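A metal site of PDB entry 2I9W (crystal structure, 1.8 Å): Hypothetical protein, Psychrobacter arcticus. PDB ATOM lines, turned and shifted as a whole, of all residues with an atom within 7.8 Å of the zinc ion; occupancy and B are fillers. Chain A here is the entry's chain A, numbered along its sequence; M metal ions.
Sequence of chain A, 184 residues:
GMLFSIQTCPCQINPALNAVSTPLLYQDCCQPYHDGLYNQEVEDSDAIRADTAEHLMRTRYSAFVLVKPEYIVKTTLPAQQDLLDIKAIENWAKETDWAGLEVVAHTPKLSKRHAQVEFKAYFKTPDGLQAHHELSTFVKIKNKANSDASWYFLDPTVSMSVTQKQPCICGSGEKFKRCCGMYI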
ATOM      1  N   THR A   8     -12.455 -13.330   7.153  1.00  0.00           N
ATOM      2  CA  THR A   8     -11.168 -13.301   7.805  1.00  0.00           C
ATOM      3  C   THR A   8     -11.041 -11.994   8.611  1.00  0.00           C
ATOM      4  O   THR A   8     -11.315 -10.869   8.126  1.00  0.00           O
ATOM      5  CB  THR A   8     -10.007 -13.529   6.795  1.00  0.00           C
ATOM      6  OG1 THR A   8     -10.231 -14.743   6.042  1.00  0.00           O
ATOM      7  CG2 THR A   8      -8.671 -13.596   7.479  1.00  0.00           C
ATOM      8  N   CYS A   9     -10.646 -12.150   9.853  1.00  0.00           N
ATOM      9  CA  CYS A   9     -10.374 -10.977  10.684  1.00  0.00           C
ATOM     10  C   CYS A   9      -9.326 -10.084   9.987  1.00  0.00           C
ATOM     11  O   CYS A   9      -8.339 -10.587   9.436  1.00  0.00           O
ATOM     12  CB  CYS A   9      -9.866 -11.372  12.051  1.00  0.00           C
ATOM     13  SG  CYS A   9      -9.889  -9.961  13.174  1.00  0.00           S
ATOM     14  N   PRO A  10      -9.522  -8.759   9.984  1.00  0.00           N
ATOM     15  CA  PRO A  10      -8.501  -7.990   9.287  1.00  0.00           C
ATOM     16  C   PRO A  10      -7.070  -8.267   9.751  1.00  0.00           C
ATOM     17  O   PRO A  10      -6.181  -8.303   8.914  1.00  0.00           O
ATOM     18  CB  PRO A  10      -8.910  -6.552   9.508  1.00  0.00           C
ATOM     19  CG  PRO A  10     -10.372  -6.602   9.705  1.00  0.00           C
ATOM     20  CD  PRO A  10     -10.643  -7.910  10.414  1.00  0.00           C
ATOM     21  N   CYS A  11      -6.867  -8.498  11.044  1.00  0.00           N
ATOM     22  CA  CYS A  11      -5.502  -8.694  11.577  1.00  0.00           C
ATOM     23  C   CYS A  11      -4.861  -9.999  11.146  1.00  0.00           C
ATOM     24  O   CYS A  11      -3.658 -10.184  11.364  1.00  0.00           O
ATOM     25  CB  CYS A  11      -5.449  -8.594  13.101  1.00  0.00           C
ATOM     26  SG  CYS A  11      -5.849 -10.099  13.944  1.00  0.00           S
ATOM     27  N   GLN A  12      -5.662 -10.883  10.559  1.00  0.00           N
ATOM     28  CA  GLN A  12      -5.223 -12.186  10.097  1.00  0.00           C
ATOM     29  C   GLN A  12      -4.847 -12.179   8.617  1.00  0.00           C
ATOM     30  O   GLN A  12      -4.389 -13.195   8.107  1.00  0.00           O
ATOM     31  CB  GLN A  12      -6.321 -13.230  10.299  1.00  0.00           C
ATOM     32  CG  GLN A  12      -6.723 -13.397  11.737  1.00  0.00           C
ATOM     33  CD  GLN A  12      -5.803 -14.303  12.490  1.00  0.00           C
ATOM     34  OE1 GLN A  12      -5.617 -15.458  12.112  1.00  0.00           O
ATOM     35  NE2 GLN A  12      -5.254 -13.801  13.591  1.00  0.00           N
ATOM     36  N   ILE A  13      -5.057 -11.050   7.947  1.00  0.00           N
ATOM     37  CA  ILE A  13      -4.614 -10.876   6.563  1.00  0.00           C
ATOM     38  C   ILE A  13      -3.133 -10.459   6.533  1.00  0.00           C
ATOM     39  O   ILE A  13      -2.771  -9.382   6.969  1.00  0.00           O
ATOM     40  CB  ILE A  13      -5.553  -9.886   5.837  1.00  0.00           C
ATOM     41  CG1 ILE A  13      -6.939 -10.554   5.732  1.00  0.00           C
ATOM     42  CG2 ILE A  13      -5.018  -9.574   4.413  1.00  0.00           C
ATOM     43  CD1 ILE A  13      -8.048  -9.649   5.554  1.00  0.00           C
ATOM     44  N   LEU A  24      -8.148 -16.811  11.183  1.00  0.00           N
ATOM     45  CA  LEU A  24      -9.382 -16.753  11.970  1.00  0.00           C
ATOM     46  C   LEU A  24     -10.357 -15.735  11.412  1.00  0.00           C
ATOM     47  O   LEU A  24      -9.957 -14.745  10.789  1.00  0.00           O
ATOM     48  CB  LEU A  24      -9.085 -16.436  13.432  1.00  0.00           C
ATOM     49  CG  LEU A  24      -8.049 -17.229  14.208  1.00  0.00           C
ATOM     50  CD1 LEU A  24      -7.907 -16.708  15.681  1.00  0.00           C
ATOM     51  CD2 LEU A  24      -8.418 -18.709  14.201  1.00  0.00           C
ATOM     52  N   LEU A  25     -11.646 -16.019  11.616  1.00  0.00           N
ATOM     53  CA  LEU A  25     -12.714 -15.058  11.314  1.00  0.00           C
ATOM     54  C   LEU A  25     -12.772 -13.938  12.324  1.00  0.00           C
ATOM     55  O   LEU A  25     -12.390 -14.088  13.502  1.00  0.00           O
ATOM     56  CB  LEU A  25     -14.080 -15.723  11.259  1.00  0.00           C
ATOM     57  CG  LEU A  25     -14.279 -16.849  10.217  1.00  0.00           C
ATOM     58  CD1 LEU A  25     -15.761 -17.316  10.189  1.00  0.00           C
ATOM     59  CD2 LEU A  25     -13.780 -16.410   8.841  1.00  0.00           C
ATOM     60  N   TYR A  26     -13.246 -12.782  11.875  1.00  0.00           N
ATOM     61  CA  TYR A  26     -13.426 -11.631  12.777  1.00  0.00           C
ATOM     62  C   TYR A  26     -14.170 -12.000  14.103  1.00  0.00           C
ATOM     63  O   TYR A  26     -13.653 -11.746  15.221  1.00  0.00           O
ATOM     64  CB  TYR A  26     -14.132 -10.520  12.015  1.00  0.00           C
ATOM     65  CG  TYR A  26     -14.420  -9.271  12.818  1.00  0.00           C
ATOM     66  CD1 TYR A  26     -13.428  -8.621  13.565  1.00  0.00           C
ATOM     67  CD2 TYR A  26     -15.700  -8.704  12.843  1.00  0.00           C
ATOM     68  CE1 TYR A  26     -13.709  -7.450  14.280  1.00  0.00           C
ATOM     69  CE2 TYR A  26     -15.984  -7.528  13.566  1.00  0.00           C
ATOM     70  CZ  TYR A  26     -14.991  -6.916  14.296  1.00  0.00           C
ATOM     71  OH  TYR A  26     -15.269  -5.769  15.010  1.00  0.00           O
ATOM     72  N   GLN A  27     -15.322 -12.661  13.990  1.00  0.00           N
ATOM     73  CA  GLN A  27     -16.082 -13.071  15.181  1.00  0.00           C
ATOM     74  C   GLN A  27     -15.275 -13.909  16.176  1.00  0.00           C
ATOM     75  O   GLN A  27     -15.594 -13.950  17.371  1.00  0.00           O
ATOM     76  CB  GLN A  27     -17.352 -13.846  14.786  1.00  0.00           C
ATOM     77  CG  GLN A  27     -17.137 -15.156  14.064  1.00  0.00           C
ATOM     78  CD  GLN A  27     -18.459 -15.808  13.600  1.00  0.00           C
ATOM     79  OE1 GLN A  27     -19.539 -15.243  13.700  1.00  0.00           O
ATOM     80  NE2 GLN A  27     -18.346 -17.007  13.071  1.00  0.00           N
ATOM     81  N   ASP A  28     -14.251 -14.584  15.675  1.00  0.00           N
ATOM     82  CA  ASP A  28     -13.452 -15.507  16.454  1.00  0.00           C
ATOM     83  C   ASP A  28     -12.129 -14.909  16.874  1.00  0.00           C
ATOM     84  O   ASP A  28     -11.319 -15.597  17.466  1.00  0.00           O
ATOM     85  CB  ASP A  28     -13.165 -16.774  15.623  1.00  0.00           C
ATOM     86  CG  ASP A  28     -14.404 -17.569  15.359  1.00  0.00           C
ATOM     87  OD1 ASP A  28     -15.214 -17.661  16.298  1.00  0.00           O
ATOM     88  OD2 ASP A  28     -14.556 -18.056  14.229  1.00  0.00           O
ATOM     89  N   CYS A  29     -11.897 -13.638  16.530  1.00  0.00           N
ATOM     90  CA  CYS A  29     -10.605 -12.979  16.756  1.00  0.00           C
ATOM     91  C   CYS A  29     -10.800 -11.605  17.434  1.00  0.00           C
ATOM     92  O   CYS A  29     -10.953 -11.555  18.654  1.00  0.00           O
ATOM     93  CB  CYS A  29      -9.805 -12.883  15.428  1.00  0.00           C
ATOM     94  SG  CYS A  29      -8.084 -12.296  15.604  1.00  0.00           S
ATOM     95  N   CYS A  30     -10.873 -10.498  16.657  1.00  0.00           N
ATOM     96  CA  CYS A  30     -10.899  -9.161  17.233  1.00  0.00           C
ATOM     97  C   CYS A  30     -12.301  -8.709  17.688  1.00  0.00           C
ATOM     98  O   CYS A  30     -12.428  -7.823  18.538  1.00  0.00           O
ATOM     99  CB  CYS A  30     -10.328  -8.189  16.196  1.00  0.00           C
ATOM    100  SG  CYS A  30      -8.488  -8.264  16.001  1.00  0.00           S
ATOM    101  N   GLN A  31     -13.371  -9.282  17.099  1.00  0.00           N
ATOM    102  CA  GLN A  31     -14.718  -8.736  17.327  1.00  0.00           C
ATOM    103  C   GLN A  31     -15.100  -8.715  18.816  1.00  0.00           C
ATOM    104  O   GLN A  31     -15.641  -7.754  19.278  1.00  0.00           O
ATOM    105  CB  GLN A  31     -15.773  -9.486  16.501  1.00  0.00           C
ATOM    106  CG  GLN A  31     -17.109  -8.857  16.641  1.00  0.00           C
ATOM    107  CD  GLN A  31     -18.145  -9.542  15.771  1.00  0.00           C
ATOM    108  OE1 GLN A  31     -17.863 -10.511  15.062  1.00  0.00           O
ATOM    109  NE2 GLN A  31     -19.355  -9.031  15.830  1.00  0.00           N
ATOM    110  N   PRO A  32     -14.788  -9.787  19.584  1.00  0.00           N
ATOM    111  CA  PRO A  32     -15.119  -9.713  21.021  1.00  0.00           C
ATOM    112  C   PRO A  32     -14.529  -8.513  21.793  1.00  0.00           C
ATOM    113  O   PRO A  32     -15.145  -8.002  22.739  1.00  0.00           O
ATOM    114  CB  PRO A  32     -14.565 -11.055  21.562  1.00  0.00           C
ATOM    115  CG  PRO A  32     -14.562 -11.949  20.371  1.00  0.00           C
ATOM    116  CD  PRO A  32     -14.183 -11.077  19.214  1.00  0.00           C
ATOM    117  N   TYR A  33     -13.347  -8.069  21.374  1.00  0.00           N
ATOM    118  CA  TYR A  33     -12.630  -7.003  22.017  1.00  0.00           C
ATOM    119  C   TYR A  33     -13.270  -5.703  21.602  1.00  0.00           C
ATOM    120  O   TYR A  33     -13.458  -4.830  22.427  1.00  0.00           O
ATOM    121  CB  TYR A  33     -11.131  -7.093  21.665  1.00  0.00           C
ATOM    122  CG  TYR A  33     -10.578  -8.378  22.192  1.00  0.00           C
ATOM    123  CD1 TYR A  33     -10.209  -8.480  23.527  1.00  0.00           C
ATOM    124  CD2 TYR A  33     -10.527  -9.502  21.420  1.00  0.00           C
ATOM    125  CE1 TYR A  33      -9.782  -9.659  24.050  1.00  0.00           C
ATOM    126  CE2 TYR A  33     -10.122 -10.722  21.941  1.00  0.00           C
ATOM    127  CZ  TYR A  33      -9.758 -10.779  23.267  1.00  0.00           C
ATOM    128  OH  TYR A  33      -9.313 -11.951  23.826  1.00  0.00           O
ATOM    129  N   HIS A  34     -13.575  -5.554  20.323  1.00  0.00           N
ATOM    130  CA  HIS A  34     -14.202  -4.309  19.891  1.00  0.00           C
ATOM    131  C   HIS A  34     -15.585  -4.199  20.610  1.00  0.00           C
ATOM    132  O   HIS A  34     -15.922  -3.194  21.219  1.00  0.00           O
ATOM    133  CB  HIS A  34     -14.435  -4.315  18.396  1.00  0.00           C
ATOM    134  CG  HIS A  34     -13.174  -4.266  17.583  1.00  0.00           C
ATOM    135  ND1 HIS A  34     -13.112  -4.669  16.269  1.00  0.00           N
ATOM    136  CD2 HIS A  34     -11.912  -3.958  17.937  1.00  0.00           C
ATOM    137  CE1 HIS A  34     -11.877  -4.510  15.831  1.00  0.00           C
ATOM    138  NE2 HIS A  34     -11.133  -4.083  16.832  1.00  0.00           N
ATOM    139  N   HIS A  55      -1.630  -8.398  21.158  1.00  0.00           N
ATOM    140  CA  HIS A  55      -3.039  -8.578  20.940  1.00  0.00           C
ATOM    141  C   HIS A  55      -3.741  -7.240  20.863  1.00  0.00           C
ATOM    142  O   HIS A  55      -4.570  -7.023  19.980  1.00  0.00           O
ATOM    143  CB  HIS A  55      -3.580  -9.471  22.033  1.00  0.00           C
ATOM    144  CG  HIS A  55      -4.956  -9.961  21.776  1.00  0.00           C
ATOM    145  ND1 HIS A  55      -5.676 -10.658  22.719  1.00  0.00           N
ATOM    146  CD2 HIS A  55      -5.754  -9.835  20.693  1.00  0.00           C
ATOM    147  CE1 HIS A  55      -6.853 -10.979  22.215  1.00  0.00           C
ATOM    148  NE2 HIS A  55      -6.932 -10.482  20.995  1.00  0.00           N
ATOM    149  N   ARG A  58      -3.103  -5.718  17.385  1.00  0.00           N
ATOM    150  CA  ARG A  58      -3.930  -6.386  16.358  1.00  0.00           C
ATOM    151  C   ARG A  58      -5.337  -5.842  16.365  1.00  0.00           C
ATOM    152  O   ARG A  58      -5.908  -5.517  15.312  1.00  0.00           O
ATOM    153  CB  ARG A  58      -3.972  -7.889  16.566  1.00  0.00           C
ATOM    154  CG  ARG A  58      -2.720  -8.554  16.133  1.00  0.00           C
ATOM    155  CD  ARG A  58      -2.680  -9.998  16.613  1.00  0.00           C
ATOM    156  NE  ARG A  58      -1.501 -10.711  16.132  1.00  0.00           N
ATOM    157  CZ  ARG A  58      -1.343 -11.214  14.902  1.00  0.00           C
ATOM    158  NH1 ARG A  58      -2.288 -11.073  13.970  1.00  0.00           N
ATOM    159  NH2 ARG A  58      -0.227 -11.861  14.611  1.00  0.00           N
ATOM    160  N   THR A  59      -5.923  -5.763  17.550  1.00  0.00           N
ATOM    161  CA  THR A  59      -7.310  -5.203  17.669  1.00  0.00           C
ATOM    162  C   THR A  59      -7.363  -3.756  17.184  1.00  0.00           C
ATOM    163  O   THR A  59      -8.370  -3.354  16.607  1.00  0.00           O
ATOM    164  CB  THR A  59      -7.915  -5.331  19.117  1.00  0.00           C
ATOM    165  OG1 THR A  59      -7.142  -4.520  20.043  1.00  0.00           O
ATOM    166  CG2 THR A  59      -7.978  -6.816  19.548  1.00  0.00           C
ATOM    167  N   TYR A  61      -5.377  -2.327  14.766  1.00  0.00           N
ATOM    168  CA  TYR A  61      -5.305  -2.478  13.314  1.00  0.00           C
ATOM    169  C   TYR A  61      -6.690  -2.838  12.717  1.00  0.00           C
ATOM    170  O   TYR A  61      -7.169  -2.201  11.799  1.00  0.00           O
ATOM    171  CB  TYR A  61      -4.273  -3.542  12.926  1.00  0.00           C
ATOM    172  CG  TYR A  61      -4.335  -3.799  11.455  1.00  0.00           C
ATOM    173  CD1 TYR A  61      -3.752  -2.949  10.575  1.00  0.00           C
ATOM    174  CD2 TYR A  61      -5.068  -4.866  10.955  1.00  0.00           C
ATOM    175  CE1 TYR A  61      -3.869  -3.123   9.187  1.00  0.00           C
ATOM    176  CE2 TYR A  61      -5.208  -5.065   9.594  1.00  0.00           C
ATOM    177  CZ  TYR A  61      -4.602  -4.173   8.692  1.00  0.00           C
ATOM    178  OH  TYR A  61      -4.703  -4.357   7.336  1.00  0.00           O
ATOM    179  N   SER A  62      -7.331  -3.840  13.305  1.00  0.00           N
ATOM    180  CA  SER A  62      -8.670  -4.263  12.839  1.00  0.00           C
ATOM    181  C   SER A  62      -9.703  -3.146  13.013  1.00  0.00           C
ATOM    182  O   SER A  62     -10.607  -3.002  12.194  1.00  0.00           O
ATOM    183  CB  SER A  62      -9.100  -5.512  13.609  1.00  0.00           C
ATOM    184  OG  SER A  62      -8.184  -6.549  13.297  1.00  0.00           O
ATOM    185  N   LEU A 101      -1.598  -6.980   7.750  1.00  0.00           N
ATOM    186  CA  LEU A 101      -0.748  -6.803   8.926  1.00  0.00           C
ATOM    187  C   LEU A 101       0.284  -7.919   9.056  1.00  0.00           C
ATOM    188  O   LEU A 101      -0.048  -9.097   8.899  1.00  0.00           O
ATOM    189  CB  LEU A 101      -1.602  -6.776  10.207  1.00  0.00           C
ATOM    190  CG  LEU A 101      -0.833  -6.574  11.527  1.00  0.00           C
ATOM    191  CD1 LEU A 101      -0.239  -5.130  11.551  1.00  0.00           C
ATOM    192  CD2 LEU A 101      -1.720  -6.919  12.776  1.00  0.00           C
HETATM  193 ZN    ZN M   1      -8.111 -10.176  14.659  1.00  0.00          ZN
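NE2 of Gln 12 sits close to SG of Cys 29.
The backbone NH of Cys 9 lies within hydrogen-bond range of the backbone carbonyl oxygen of Leu 24, at 2.8 Å.
The side-chain sulfur of Cys 30 sits close to the side-chain hydroxyl of Ser 62 (3.2 Å).
The backbone NH (N) of Cys 11 is in hydrogen-bond range of the side-chain hydroxyl (OG) of Ser 62, at 3.3 Å.
The side-chain sulfur (SG) of Cys 11 lies close to the side-chain amide nitrogen (NE2) of Gln 12, at 3.8 Å.
The backbone carbonyl oxygen (O) of Cys 11 is in hydrogen-bond range of the guanidinium group (NH1) of Arg 58, at 3.1 Å.
The side-chain hydroxyl (OG) of Ser 62 sits at hydrogen-bond distance from the backbone carbonyl oxygen (O) of Arg 58, 3.2 Å away.
The zinc ion is bound by SG of Cys 29 (2.3 Å).
The side-chain sulfur (SG) of Cys 9 is bound to the zinc ion (2.3 Å).
The side-chain sulfur (SG) of Cys 30 is bound to the zinc ion.
The zinc ion is bound by the side-chain sulfur (SG) of Cys 11, 2.4 Å away.
Ser 62 touches the zinc ion.
Five residues have an atom within 4 Å of the zinc ion: Cys 9, Cys 11, Cys 29, Cys 30 and Ser 62.
The nearest printed residue that does not touch the zinc ion is Gln 12 (4.6 Å).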
